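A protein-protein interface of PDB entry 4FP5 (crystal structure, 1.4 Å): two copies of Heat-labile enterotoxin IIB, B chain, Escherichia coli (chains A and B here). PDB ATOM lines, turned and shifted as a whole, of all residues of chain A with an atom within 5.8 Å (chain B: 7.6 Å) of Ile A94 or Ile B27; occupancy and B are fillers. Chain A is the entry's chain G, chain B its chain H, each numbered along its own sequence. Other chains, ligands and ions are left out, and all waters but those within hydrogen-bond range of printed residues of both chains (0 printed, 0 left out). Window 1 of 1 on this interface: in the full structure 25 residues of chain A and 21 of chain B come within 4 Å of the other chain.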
ATOM      1  N   SER A   3      22.444 -15.103  -6.026  1.00  0.00           N
ATOM      2  CA  SER A   3      23.384 -16.111  -6.462  1.00  0.00           C
ATOM      3  C   SER A   3      24.122 -16.664  -5.249  1.00  0.00           C
ATOM      4  O   SER A   3      24.339 -16.043  -4.248  1.00  0.00           O
ATOM      5  CB  SER A   3      24.365 -15.451  -7.423  1.00  0.00           C
ATOM      6  OG  SER A   3      25.188 -14.468  -6.809  1.00  0.00           O
ATOM      7  N   PHE A   5      27.223 -17.162  -5.227  1.00  0.00           N
ATOM      8  CA  PHE A   5      28.357 -16.286  -5.049  1.00  0.00           C
ATOM      9  C   PHE A   5      28.091 -15.055  -4.108  1.00  0.00           C
ATOM     10  O   PHE A   5      28.828 -14.739  -3.142  1.00  0.00           O
ATOM     11  CB  PHE A   5      28.755 -15.773  -6.504  1.00  0.00           C
ATOM     12  CG  PHE A   5      29.882 -14.819  -6.500  1.00  0.00           C
ATOM     13  CD1 PHE A   5      31.197 -15.225  -6.290  1.00  0.00           C
ATOM     14  CD2 PHE A   5      29.614 -13.442  -6.787  1.00  0.00           C
ATOM     15  CE1 PHE A   5      32.258 -14.301  -6.338  1.00  0.00           C
ATOM     16  CE2 PHE A   5      30.662 -12.563  -6.796  1.00  0.00           C
ATOM     17  CZ  PHE A   5      31.951 -12.965  -6.604  1.00  0.00           C
ATOM     18  N   PHE A   6      26.931 -14.402  -4.438  1.00  0.00           N
ATOM     19  CA  PHE A   6      26.600 -13.234  -3.604  1.00  0.00           C
ATOM     20  C   PHE A   6      26.356 -13.602  -2.076  1.00  0.00           C
ATOM     21  O   PHE A   6      26.806 -12.938  -1.205  1.00  0.00           O
ATOM     22  CB  PHE A   6      25.357 -12.587  -4.207  1.00  0.00           C
ATOM     23  CG  PHE A   6      25.018 -11.258  -3.603  1.00  0.00           C
ATOM     24  CD1 PHE A   6      25.649 -10.072  -4.053  1.00  0.00           C
ATOM     25  CD2 PHE A   6      24.029 -11.151  -2.603  1.00  0.00           C
ATOM     26  CE1 PHE A   6      25.322  -8.862  -3.533  1.00  0.00           C
ATOM     27  CE2 PHE A   6      23.682  -9.919  -2.078  1.00  0.00           C
ATOM     28  CZ  PHE A   6      24.337  -8.763  -2.518  1.00  0.00           C
ATOM     29  N   LEU A  23      12.427  -2.407  -4.920  1.00  0.00           N
ATOM     30  CA  LEU A  23      12.659  -1.005  -4.631  1.00  0.00           C
ATOM     31  C   LEU A  23      11.705  -0.182  -5.417  1.00  0.00           C
ATOM     32  O   LEU A  23      11.634  -0.285  -6.641  1.00  0.00           O
ATOM     33  CB  LEU A  23      14.097  -0.651  -5.030  1.00  0.00           C
ATOM     34  CG  LEU A  23      15.114  -1.396  -4.195  1.00  0.00           C
ATOM     35  CD1 LEU A  23      16.529  -0.952  -4.646  1.00  0.00           C
ATOM     36  CD2 LEU A  23      14.950  -1.207  -2.691  1.00  0.00           C
ATOM     37  N   GLU A  63      28.150   2.323  -9.232  1.00  0.00           N
ATOM     38  CA  GLU A  63      27.340   1.279  -9.833  1.00  0.00           C
ATOM     39  C   GLU A  63      26.173   0.928  -8.897  1.00  0.00           C
ATOM     40  O   GLU A  63      25.137   0.532  -9.401  1.00  0.00           O
ATOM     41  CB  GLU A  63      28.201   0.047 -10.146  1.00  0.00           C
ATOM     42  CG  GLU A  63      29.324   0.393 -11.208  1.00  0.00           C
ATOM     43  CD  GLU A  63      28.737   0.866 -12.506  1.00  0.00           C
ATOM     44  OE1 GLU A  63      27.831   0.242 -13.044  1.00  0.00           O
ATOM     45  OE2 GLU A  63      29.310   1.892 -13.014  1.00  0.00           O
ATOM     46  N   MET A  64      26.380   1.003  -7.588  1.00  0.00           N
ATOM     47  CA  MET A  64      25.236   0.740  -6.648  1.00  0.00           C
ATOM     48  C   MET A  64      24.164   1.769  -6.959  1.00  0.00           C
ATOM     49  O   MET A  64      22.970   1.411  -6.961  1.00  0.00           O
ATOM     50  CB  MET A  64      25.657   0.900  -5.191  1.00  0.00           C
ATOM     51  CG  MET A  64      26.575  -0.129  -4.691  1.00  0.00           C
ATOM     52  SD  MET A  64      26.835   0.119  -2.933  1.00  0.00           S
ATOM     53  CE  MET A  64      27.871  -1.318  -2.556  1.00  0.00           C
ATOM     54  N   ILE A  67      22.465   0.678 -10.180  1.00  0.00           N
ATOM     55  CA  ILE A  67      21.608  -0.492  -9.892  1.00  0.00           C
ATOM     56  C   ILE A  67      20.338  -0.039  -9.221  1.00  0.00           C
ATOM     57  O   ILE A  67      19.243  -0.465  -9.634  1.00  0.00           O
ATOM     58  CB  ILE A  67      22.393  -1.461  -9.089  1.00  0.00           C
ATOM     59  CG1 ILE A  67      23.414  -2.177  -9.957  1.00  0.00           C
ATOM     60  CG2 ILE A  67      21.461  -2.492  -8.431  1.00  0.00           C
ATOM     61  CD1 ILE A  67      24.564  -2.900  -9.189  1.00  0.00           C
ATOM     62  N   ALA A  68      20.413   0.830  -8.214  1.00  0.00           N
ATOM     63  CA  ALA A  68      19.201   1.260  -7.456  1.00  0.00           C
ATOM     64  C   ALA A  68      18.288   1.988  -8.421  1.00  0.00           C
ATOM     65  O   ALA A  68      17.058   1.708  -8.478  1.00  0.00           O
ATOM     66  CB  ALA A  68      19.655   2.231  -6.347  1.00  0.00           C
ATOM     67  N   VAL A  78      16.211  -6.712  -6.292  1.00  0.00           N
ATOM     68  CA  VAL A  78      17.585  -6.756  -5.894  1.00  0.00           C
ATOM     69  C   VAL A  78      17.832  -7.614  -4.689  1.00  0.00           C
ATOM     70  O   VAL A  78      16.908  -7.817  -3.870  1.00  0.00           O
ATOM     71  CB  VAL A  78      18.169  -5.348  -5.565  1.00  0.00           C
ATOM     72  CG1 VAL A  78      18.044  -4.437  -6.748  1.00  0.00           C
ATOM     73  CG2 VAL A  78      17.503  -4.681  -4.336  1.00  0.00           C
ATOM     74  N   ASN A  79      19.030  -8.139  -4.546  1.00  0.00           N
ATOM     75  CA  ASN A  79      19.494  -8.736  -3.303  1.00  0.00           C
ATOM     76  C   ASN A  79      20.519  -7.873  -2.655  1.00  0.00           C
ATOM     77  O   ASN A  79      21.320  -7.254  -3.354  1.00  0.00           O
ATOM     78  CB  ASN A  79      20.053 -10.160  -3.572  1.00  0.00           C
ATOM     79  CG  ASN A  79      19.099 -10.973  -4.443  1.00  0.00           C
ATOM     80  OD1 ASN A  79      17.939 -11.165  -4.068  1.00  0.00           O
ATOM     81  ND2 ASN A  79      19.532 -11.364  -5.616  1.00  0.00           N
ATOM     82  N   MET A  80      20.502  -7.697  -1.347  1.00  0.00           N
ATOM     83  CA  MET A  80      21.392  -6.805  -0.626  1.00  0.00           C
ATOM     84  C   MET A  80      22.229  -7.483   0.406  1.00  0.00           C
ATOM     85  O   MET A  80      21.672  -8.364   1.100  1.00  0.00           O
ATOM     86  CB  MET A  80      20.684  -5.600   0.004  1.00  0.00           C
ATOM     87  CG  MET A  80      20.070  -4.717  -1.099  1.00  0.00           C
ATOM     88  SD  MET A  80      19.166  -3.188  -0.729  1.00  0.00           S
ATOM     89  CE  MET A  80      17.710  -4.033  -0.131  1.00  0.00           C
ATOM     90  N   CYS A  81      23.424  -7.011   0.635  1.00  0.00           N
ATOM     91  CA  CYS A  81      24.177  -7.357   1.817  1.00  0.00           C
ATOM     92  C   CYS A  81      24.229  -6.090   2.575  1.00  0.00           C
ATOM     93  O   CYS A  81      24.880  -5.122   2.175  1.00  0.00           O
ATOM     94  CB  CYS A  81      25.594  -7.745   1.386  1.00  0.00           C
ATOM     95  SG  CYS A  81      26.608  -8.314   2.756  1.00  0.00           S
ATOM     96  N   ILE A  91      23.933  -0.423   2.534  1.00  0.00           N
ATOM     97  CA  ILE A  91      24.177  -1.452   1.553  1.00  0.00           C
ATOM     98  C   ILE A  91      25.699  -1.556   1.275  1.00  0.00           C
ATOM     99  O   ILE A  91      26.305  -0.573   0.762  1.00  0.00           O
ATOM    100  CB  ILE A  91      23.415  -1.085   0.257  1.00  0.00           C
ATOM    101  CG1 ILE A  91      21.941  -1.048   0.511  1.00  0.00           C
ATOM    102  CG2 ILE A  91      23.775  -2.104  -0.865  1.00  0.00           C
ATOM    103  CD1 ILE A  91      21.179  -0.316  -0.589  1.00  0.00           C
ATOM    104  N   TRP A  92      26.276  -2.721   1.599  1.00  0.00           N
ATOM    105  CA  TRP A  92      27.688  -2.946   1.330  1.00  0.00           C
ATOM    106  C   TRP A  92      27.856  -3.765   0.075  1.00  0.00           C
ATOM    107  O   TRP A  92      28.954  -3.788  -0.510  1.00  0.00           O
ATOM    108  CB  TRP A  92      28.316  -3.716   2.493  1.00  0.00           C
ATOM    109  CG  TRP A  92      28.504  -2.901   3.744  1.00  0.00           C
ATOM    110  CD1 TRP A  92      28.248  -1.597   3.959  1.00  0.00           C
ATOM    111  CD2 TRP A  92      28.862  -3.463   5.069  1.00  0.00           C
ATOM    112  NE1 TRP A  92      28.580  -1.240   5.281  1.00  0.00           N
ATOM    113  CE2 TRP A  92      28.908  -2.317   5.961  1.00  0.00           C
ATOM    114  CE3 TRP A  92      29.147  -4.788   5.563  1.00  0.00           C
ATOM    115  CZ2 TRP A  92      29.266  -2.461   7.304  1.00  0.00           C
ATOM    116  CZ3 TRP A  92      29.474  -4.900   6.918  1.00  0.00           C
ATOM    117  CH2 TRP A  92      29.582  -3.777   7.721  1.00  0.00           C
ATOM    118  N   ALA A  93      26.828  -4.477  -0.389  1.00  0.00           N
ATOM    119  CA  ALA A  93      26.861  -5.130  -1.692  1.00  0.00           C
ATOM    120  C   ALA A  93      25.474  -5.212  -2.188  1.00  0.00           C
ATOM    121  O   ALA A  93      24.493  -5.351  -1.392  1.00  0.00           O
ATOM    122  CB  ALA A  93      27.528  -6.518  -1.603  1.00  0.00           C
ATOM    123  N   ILE A  94      25.247  -5.159  -3.489  1.00  0.00           N
ATOM    124  CA  ILE A  94      23.924  -5.264  -4.084  1.00  0.00           C
ATOM    125  C   ILE A  94      24.004  -6.062  -5.369  1.00  0.00           C
ATOM    126  O   ILE A  94      25.014  -5.956  -6.114  1.00  0.00           O
ATOM    127  CB  ILE A  94      23.295  -3.871  -4.284  1.00  0.00           C
ATOM    128  CG1 ILE A  94      21.830  -3.940  -4.718  1.00  0.00           C
ATOM    129  CG2 ILE A  94      24.147  -3.024  -5.250  1.00  0.00           C
ATOM    130  CD1 ILE A  94      21.123  -2.604  -4.504  1.00  0.00           C
ATOM    131  N   GLU A  95      22.984  -6.853  -5.658  1.00  0.00           N
ATOM    132  CA  GLU A  95      22.816  -7.675  -6.848  1.00  0.00           C
ATOM    133  C   GLU A  95      21.581  -7.354  -7.513  1.00  0.00           C
ATOM    134  O   GLU A  95      20.496  -7.588  -6.956  1.00  0.00           O
ATOM    135  CB  GLU A  95      22.925  -9.167  -6.432  1.00  0.00           C
ATOM    136  CG  GLU A  95      22.737 -10.159  -7.568  1.00  0.00           C
ATOM    137  CD  GLU A  95      23.008 -11.583  -7.096  1.00  0.00           C
ATOM    138  OE1 GLU A  95      22.204 -12.132  -6.283  1.00  0.00           O
ATOM    139  OE2 GLU A  95      24.071 -12.157  -7.470  1.00  0.00           O
ATOM    140  N   LEU A  96      21.653  -6.859  -8.742  1.00  0.00           N
ATOM    141  CA  LEU A  96      20.487  -6.661  -9.561  1.00  0.00           C
ATOM    142  C   LEU A  96      20.120  -7.916 -10.272  1.00  0.00           C
ATOM    143  O   LEU A  96      20.975  -8.554 -10.857  1.00  0.00           O
ATOM    144  CB  LEU A  96      20.835  -5.590 -10.623  1.00  0.00           C
ATOM    145  CG  LEU A  96      19.738  -5.187 -11.626  1.00  0.00           C
ATOM    146  CD1 LEU A  96      18.563  -4.511 -10.918  1.00  0.00           C
ATOM    147  CD2 LEU A  96      20.318  -4.285 -12.736  1.00  0.00           C
ATOM    148  N   LYS B  25      22.508 -11.412 -13.589  1.00  0.00           N
ATOM    149  CA  LYS B  25      22.708 -10.655 -12.362  1.00  0.00           C
ATOM    150  C   LYS B  25      23.924  -9.736 -12.509  1.00  0.00           C
ATOM    151  O   LYS B  25      24.933 -10.102 -13.205  1.00  0.00           O
ATOM    152  CB  LYS B  25      22.963 -11.543 -11.175  1.00  0.00           C
ATOM    153  CG  LYS B  25      21.845 -12.577 -11.104  1.00  0.00           C
ATOM    154  CD  LYS B  25      22.054 -13.475  -9.881  1.00  0.00           C
ATOM    155  CE  LYS B  25      20.958 -14.518  -9.595  1.00  0.00           C
ATOM    156  NZ  LYS B  25      19.533 -14.190  -9.737  1.00  0.00           N
ATOM    157  N   TYR B  26      23.883  -8.576 -11.830  1.00  0.00           N
ATOM    158  CA  TYR B  26      24.999  -7.601 -11.836  1.00  0.00           C
ATOM    159  C   TYR B  26      25.256  -7.213 -10.405  1.00  0.00           C
ATOM    160  O   TYR B  26      24.327  -6.795  -9.682  1.00  0.00           O
ATOM    161  CB  TYR B  26      24.524  -6.404 -12.744  1.00  0.00           C
ATOM    162  CG  TYR B  26      25.544  -5.299 -12.916  1.00  0.00           C
ATOM    163  CD1 TYR B  26      26.882  -5.562 -13.265  1.00  0.00           C
ATOM    164  CD2 TYR B  26      25.209  -4.014 -12.720  1.00  0.00           C
ATOM    165  CE1 TYR B  26      27.777  -4.526 -13.523  1.00  0.00           C
ATOM    166  CE2 TYR B  26      26.114  -2.984 -12.897  1.00  0.00           C
ATOM    167  CZ  TYR B  26      27.372  -3.226 -13.324  1.00  0.00           C
ATOM    168  OH  TYR B  26      28.304  -2.240 -13.611  1.00  0.00           O
ATOM    169  N   ILE B  27      26.469  -7.332  -9.954  1.00  0.00           N
ATOM    170  CA  ILE B  27      26.805  -7.159  -8.529  1.00  0.00           C
ATOM    171  C   ILE B  27      27.832  -6.057  -8.360  1.00  0.00           C
ATOM    172  O   ILE B  27      28.874  -6.042  -9.071  1.00  0.00           O
ATOM    173  CB  ILE B  27      27.412  -8.454  -7.957  1.00  0.00           C
ATOM    174  CG1 ILE B  27      26.376  -9.625  -8.061  1.00  0.00           C
ATOM    175  CG2 ILE B  27      27.970  -8.261  -6.580  1.00  0.00           C
ATOM    176  CD1 ILE B  27      27.077 -10.985  -7.861  1.00  0.00           C
ATOM    177  N   SER B  28      27.592  -5.173  -7.388  1.00  0.00           N
ATOM    178  CA  SER B  28      28.604  -4.282  -6.879  1.00  0.00           C
ATOM    179  C   SER B  28      28.867  -4.542  -5.430  1.00  0.00           C
ATOM    180  O   SER B  28      27.880  -4.657  -4.655  1.00  0.00           O
ATOM    181  CB  SER B  28      28.105  -2.832  -7.037  1.00  0.00           C
ATOM    182  OG  SER B  28      29.053  -1.958  -6.435  1.00  0.00           O
ATOM    183  N   ASP B  29      30.091  -4.750  -5.048  1.00  0.00           N
ATOM    184  CA  ASP B  29      30.400  -5.139  -3.640  1.00  0.00           C
ATOM    185  C   ASP B  29      31.568  -4.268  -3.156  1.00  0.00           C
ATOM    186  O   ASP B  29      32.583  -4.156  -3.879  1.00  0.00           O
ATOM    187  CB  ASP B  29      30.773  -6.594  -3.726  1.00  0.00           C
ATOM    188  CG  ASP B  29      31.091  -7.250  -2.376  1.00  0.00           C
ATOM    189  OD1 ASP B  29      31.201  -6.564  -1.320  1.00  0.00           O
ATOM    190  OD2 ASP B  29      30.971  -8.530  -2.284  1.00  0.00           O
ATOM    191  N   ILE B  30      31.451  -3.682  -1.942  1.00  0.00           N
ATOM    192  CA  ILE B  30      32.581  -2.999  -1.348  1.00  0.00           C
ATOM    193  C   ILE B  30      33.140  -3.645  -0.089  1.00  0.00           C
ATOM    194  O   ILE B  30      33.992  -3.041   0.576  1.00  0.00           O
ATOM    195  CB  ILE B  30      32.328  -1.514  -1.083  1.00  0.00           C
ATOM    196  CG1 ILE B  30      31.112  -1.260  -0.166  1.00  0.00           C
ATOM    197  CG2 ILE B  30      32.061  -0.776  -2.399  1.00  0.00           C
ATOM    198  CD1 ILE B  30      31.207  -1.798   1.267  1.00  0.00           C
ATOM    199  N   ASN B  31      32.716  -4.853   0.168  1.00  0.00           N
ATOM    200  CA  ASN B  31      33.253  -5.588   1.364  1.00  0.00           C
ATOM    201  C   ASN B  31      34.720  -5.891   1.247  1.00  0.00           C
ATOM    202  O   ASN B  31      35.223  -6.144   0.145  1.00  0.00           O
ATOM    203  CB  ASN B  31      32.406  -6.799   1.660  1.00  0.00           C
ATOM    204  CG  ASN B  31      31.069  -6.426   2.305  1.00  0.00           C
ATOM    205  OD1 ASN B  31      31.036  -5.631   3.258  1.00  0.00           O
ATOM    206  ND2 ASN B  31      30.015  -7.015   1.821  1.00  0.00           N
ATOM    207  N   THR B  34      36.172  -9.109  -0.945  1.00  0.00           N
ATOM    208  CA  THR B  34      35.343  -9.560  -2.039  1.00  0.00           C
ATOM    209  C   THR B  34      34.920  -8.331  -2.862  1.00  0.00           C
ATOM    210  O   THR B  34      34.044  -8.470  -3.727  1.00  0.00           O
ATOM    211  CB  THR B  34      34.091 -10.340  -1.624  1.00  0.00           C
ATOM    212  OG1 THR B  34      33.257  -9.534  -0.748  1.00  0.00           O
ATOM    213  CG2 THR B  34      34.510 -11.617  -0.793  1.00  0.00           C
ATOM    214  N   GLY B  36      34.380  -5.562  -5.624  1.00  0.00           N
ATOM    215  CA  GLY B  36      34.540  -5.567  -7.088  1.00  0.00           C
ATOM    216  C   GLY B  36      33.191  -5.504  -7.743  1.00  0.00           C
ATOM    217  O   GLY B  36      32.137  -5.376  -7.086  1.00  0.00           O
ATOM    218  N   MET B  37      33.205  -5.489  -9.066  1.00  0.00           N
ATOM    219  CA  MET B  37      32.044  -5.593  -9.915  1.00  0.00           C
ATOM    220  C   MET B  37      32.018  -6.963 -10.584  1.00  0.00           C
ATOM    221  O   MET B  37      33.004  -7.398 -11.125  1.00  0.00           O
ATOM    222  CB  MET B  37      32.069  -4.487 -11.018  1.00  0.00           C
ATOM    223  CG  MET B  37      32.085  -3.071 -10.506  1.00  0.00           C
ATOM    224  SD  MET B  37      30.598  -2.696  -9.536  1.00  0.00           S
ATOM    225  CE  MET B  37      29.329  -3.268 -10.675  1.00  0.00           C
ATOM    226  N   TYR B  38      30.867  -7.593 -10.576  1.00  0.00           N
ATOM    227  CA  TYR B  38      30.745  -8.941 -11.053  1.00  0.00           C
ATOM    228  C   TYR B  38      29.474  -9.117 -11.833  1.00  0.00           C
ATOM    229  O   TYR B  38      28.456  -8.381 -11.687  1.00  0.00           O
ATOM    230  CB  TYR B  38      30.788 -10.024  -9.945  1.00  0.00           C
ATOM    231  CG  TYR B  38      31.849  -9.858  -8.957  1.00  0.00           C
ATOM    232  CD1 TYR B  38      31.656  -9.102  -7.804  1.00  0.00           C
ATOM    233  CD2 TYR B  38      33.060 -10.528  -9.124  1.00  0.00           C
ATOM    234  CE1 TYR B  38      32.616  -9.027  -6.814  1.00  0.00           C
ATOM    235  CE2 TYR B  38      34.057 -10.462  -8.180  1.00  0.00           C
ATOM    236  CZ  TYR B  38      33.840  -9.676  -7.033  1.00  0.00           C
ATOM    237  OH  TYR B  38      34.832  -9.624  -6.024  1.00  0.00           O
ATOM    238  N   VAL B  39      29.497 -10.113 -12.759  1.00  0.00           N
ATOM    239  CA  VAL B  39      28.284 -10.510 -13.450  1.00  0.00           C
ATOM    240  C   VAL B  39      28.054 -12.019 -13.258  1.00  0.00           C
ATOM    241  O   VAL B  39      29.022 -12.769 -13.105  1.00  0.00           O
ATOM    242  CB  VAL B  39      28.296 -10.191 -14.978  1.00  0.00           C
ATOM    243  CG1 VAL B  39      28.208  -8.685 -15.117  1.00  0.00           C
ATOM    244  CG2 VAL B  39      29.519 -10.799 -15.690  1.00  0.00           C
ATOM    245  N   VAL B  40      26.790 -12.436 -13.268  1.00  0.00           N
ATOM    246  CA  VAL B  40      26.470 -13.875 -13.116  1.00  0.00           C
ATOM    247  C   VAL B  40      25.578 -14.211 -14.252  1.00  0.00           C
ATOM    248  O   VAL B  40      24.688 -13.448 -14.682  1.00  0.00           O
ATOM    249  CB  VAL B  40      25.681 -14.110 -11.775  1.00  0.00           C
ATOM    250  CG1 VAL B  40      25.443 -15.605 -11.556  1.00  0.00           C
ATOM    251  CG2 VAL B  40      26.438 -13.571 -10.582  1.00  0.00           C
ATOM    252  N   VAL B  46      30.143 -16.947 -12.948  1.00  0.00           N
ATOM    253  CA  VAL B  46      30.502 -15.661 -12.337  1.00  0.00           C
ATOM    254  C   VAL B  46      31.792 -15.156 -12.962  1.00  0.00           C
ATOM    255  O   VAL B  46      32.757 -15.874 -13.143  1.00  0.00           O
ATOM    256  CB  VAL B  46      30.815 -15.745 -10.819  1.00  0.00           C
ATOM    257  CG1 VAL B  46      30.966 -14.376 -10.195  1.00  0.00           C
ATOM    258  CG2 VAL B  46      29.606 -16.353 -10.101  1.00  0.00           C
ATOM    259  N   TRP B  47      31.785 -13.862 -13.294  1.00  0.00           N
ATOM    260  CA  TRP B  47      32.989 -13.172 -13.779  1.00  0.00           C
ATOM    261  C   TRP B  47      33.184 -11.856 -13.120  1.00  0.00           C
ATOM    262  O   TRP B  47      32.199 -11.196 -12.713  1.00  0.00           O
ATOM    263  CB  TRP B  47      32.862 -12.867 -15.335  1.00  0.00           C
ATOM    264  CG  TRP B  47      32.856 -14.106 -16.199  1.00  0.00           C
ATOM    265  CD1 TRP B  47      33.998 -14.674 -16.843  1.00  0.00           C
ATOM    266  CD2 TRP B  47      31.722 -14.967 -16.556  1.00  0.00           C
ATOM    267  NE1 TRP B  47      33.586 -15.833 -17.516  1.00  0.00           N
ATOM    268  CE2 TRP B  47      32.250 -16.041 -17.389  1.00  0.00           C
ATOM    269  CE3 TRP B  47      30.357 -14.971 -16.228  1.00  0.00           C
ATOM    270  CZ2 TRP B  47      31.422 -17.022 -17.893  1.00  0.00           C
ATOM    271  CZ3 TRP B  47      29.552 -15.962 -16.733  1.00  0.00           C
ATOM    272  CH2 TRP B  47      30.082 -16.993 -17.517  1.00  0.00           C
ATOM    273  N   ILE B  49      34.474  -8.025 -13.526  1.00  0.00           N
ATOM    274  CA  ILE B  49      34.763  -7.021 -14.568  1.00  0.00           C
ATOM    275  C   ILE B  49      36.069  -6.342 -14.236  1.00  0.00           C
ATOM    276  O   ILE B  49      36.373  -5.994 -13.106  1.00  0.00           O
ATOM    277  CB  ILE B  49      33.625  -5.963 -14.610  1.00  0.00           C
ATOM    278  CG1 ILE B  49      32.328  -6.676 -14.895  1.00  0.00           C
ATOM    279  CG2 ILE B  49      33.956  -4.997 -15.761  1.00  0.00           C
ATOM    280  CD1 ILE B  49      31.144  -5.753 -14.906  1.00  0.00           C
ATOM    281  N   ALA B  68      27.706  -4.614 -19.307  1.00  0.00           N
ATOM    282  CA  ALA B  68      27.147  -5.609 -18.394  1.00  0.00           C
ATOM    283  C   ALA B  68      25.837  -5.205 -17.930  1.00  0.00           C
ATOM    284  O   ALA B  68      24.837  -6.026 -17.933  1.00  0.00           O
ATOM    285  CB  ALA B  68      28.045  -5.714 -17.188  1.00  0.00           C
ATOM    286  N   VAL B  72      22.214  -7.244 -18.801  1.00  0.00           N
ATOM    287  CA  VAL B  72      21.314  -7.740 -17.733  1.00  0.00           C
ATOM    288  C   VAL B  72      19.949  -7.087 -17.869  1.00  0.00           C
ATOM    289  O   VAL B  72      18.916  -7.765 -17.834  1.00  0.00           O
ATOM    290  CB  VAL B  72      21.926  -7.437 -16.346  1.00  0.00           C
ATOM    291  CG1 VAL B  72      20.911  -7.717 -15.209  1.00  0.00           C
ATOM    292  CG2 VAL B  72      23.123  -8.296 -16.121  1.00  0.00           C
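OE1 of Glu A63 sits at hydrogen-bond distance from OH of Tyr B26.
The side-chain sulfur (SG) of Cys A81 lies within hydrogen-bond range of the side-chain amide nitrogen (ND2) of Asn B31, at 3.8 Å.
The backbone carbonyl oxygen (O) of Trp A92 lies within hydrogen-bond range of the backbone NH (N) of Ile B30 (2.9 Å).
N of Ile A94 sits at hydrogen-bond distance from O of Ser B28 (2.9 Å).
O of Tyr B26 sits at hydrogen-bond distance from N of Leu A96 (2.8 Å).
The side-chain hydroxyl of Ser A3 is in hydrogen-bond range of the side-chain carboxylate of Glu A95.
O of Ala A93 lies within hydrogen-bond range of N of Cys A81 (2.8 Å).
O of Lys B25 lies within hydrogen-bond range of N of Val B40, 3.0 Å away.
The side-chain sulfur (SD) of Met B37 lies close to the side-chain hydroxyl (OG) of Ser B28, 3.5 Å away.
The side-chain hydroxyl (OG1) of Thr B34 is in hydrogen-bond range of the side-chain carboxylate (OD2) of Asp B29, at 2.9 Å.
The backbone carbonyl oxygen of Met B37 is in hydrogen-bond range of the backbone NH of Ile B49 (2.9 Å).
Among the printed residues, merely in contact across the chains: Trp A92 with Asn B31 (3.1 Å), Leu A96 with Lys B25 (3.1 Å), Ala A93 with Ser B28 (3.2 Å), Ile A94 with Ile B27 (3.2 Å), Glu A95 with Ile B27 (3.3 Å), Glu A95 with Tyr B26 (3.3 Å), Glu A95 with Lys B25 (3.4 Å), Met A64 with Ser B28 (3.5 Å), Glu A63 with Met B37 (3.5 Å), Phe A5 with Tyr B38 (3.6 Å), Trp A92 with Asp B29 (3.7 Å), Ala A93 with Asp B29 (3.7 Å), Phe A5 with Ile B27 (3.7 Å), Ile A94 with Tyr B26 (3.7 Å), Phe A5 with Val B46 (3.7 Å), Ile A67 with Tyr B26 (3.8 Å), Phe A6 with Ile B27 (3.9 Å) and Ser A3 with Lys B25 (3.9 Å).
Of the printed residues of chain B, Ser A3 touches Lys B25 (3.9 Å).
Printed residues of chain B within 4 Å of Met A64: Ser B28 (3.5 Å).
Of chain B, only Ser B28 (3.2 Å) and Asp B29 (3.7 Å) come within 4 Å of Ala A93.
Ile A94 touches just these residues of chain B: Tyr B26, Ile B27 and Ser B28.
Printed residues of chain B within 4 Å of Leu A96: Lys B25 and Tyr B26.
Ile B27 touches just these residues of chain A: Phe A5 (3.7 Å), Phe A6 (3.9 Å), Ile A94 (3.2 Å) and Glu A95 (3.3 Å).
Of the printed residues of chain A, Tyr B38 touches Phe A5 (3.6 Å).
Of the 18 printed residues of chain A, 12 touch a printed residue of chain B.
Hydrophobic or aromatic side chains of chain A that line the printed part of chain B: Phe A5, Phe A6, Met A64, Ile A67, Trp A92, Ala A93 and Leu A96.
Of the 18 printed residues of chain B, 10 touch a printed residue of chain A.
Among the printed residues, 23 pairs touch across the chains.
Among the printed residues, no Asp or Glu carboxylate lies within 4 Å of a Lys or Arg side-chain nitrogen of the other chain.
1 position is printed for both chains.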
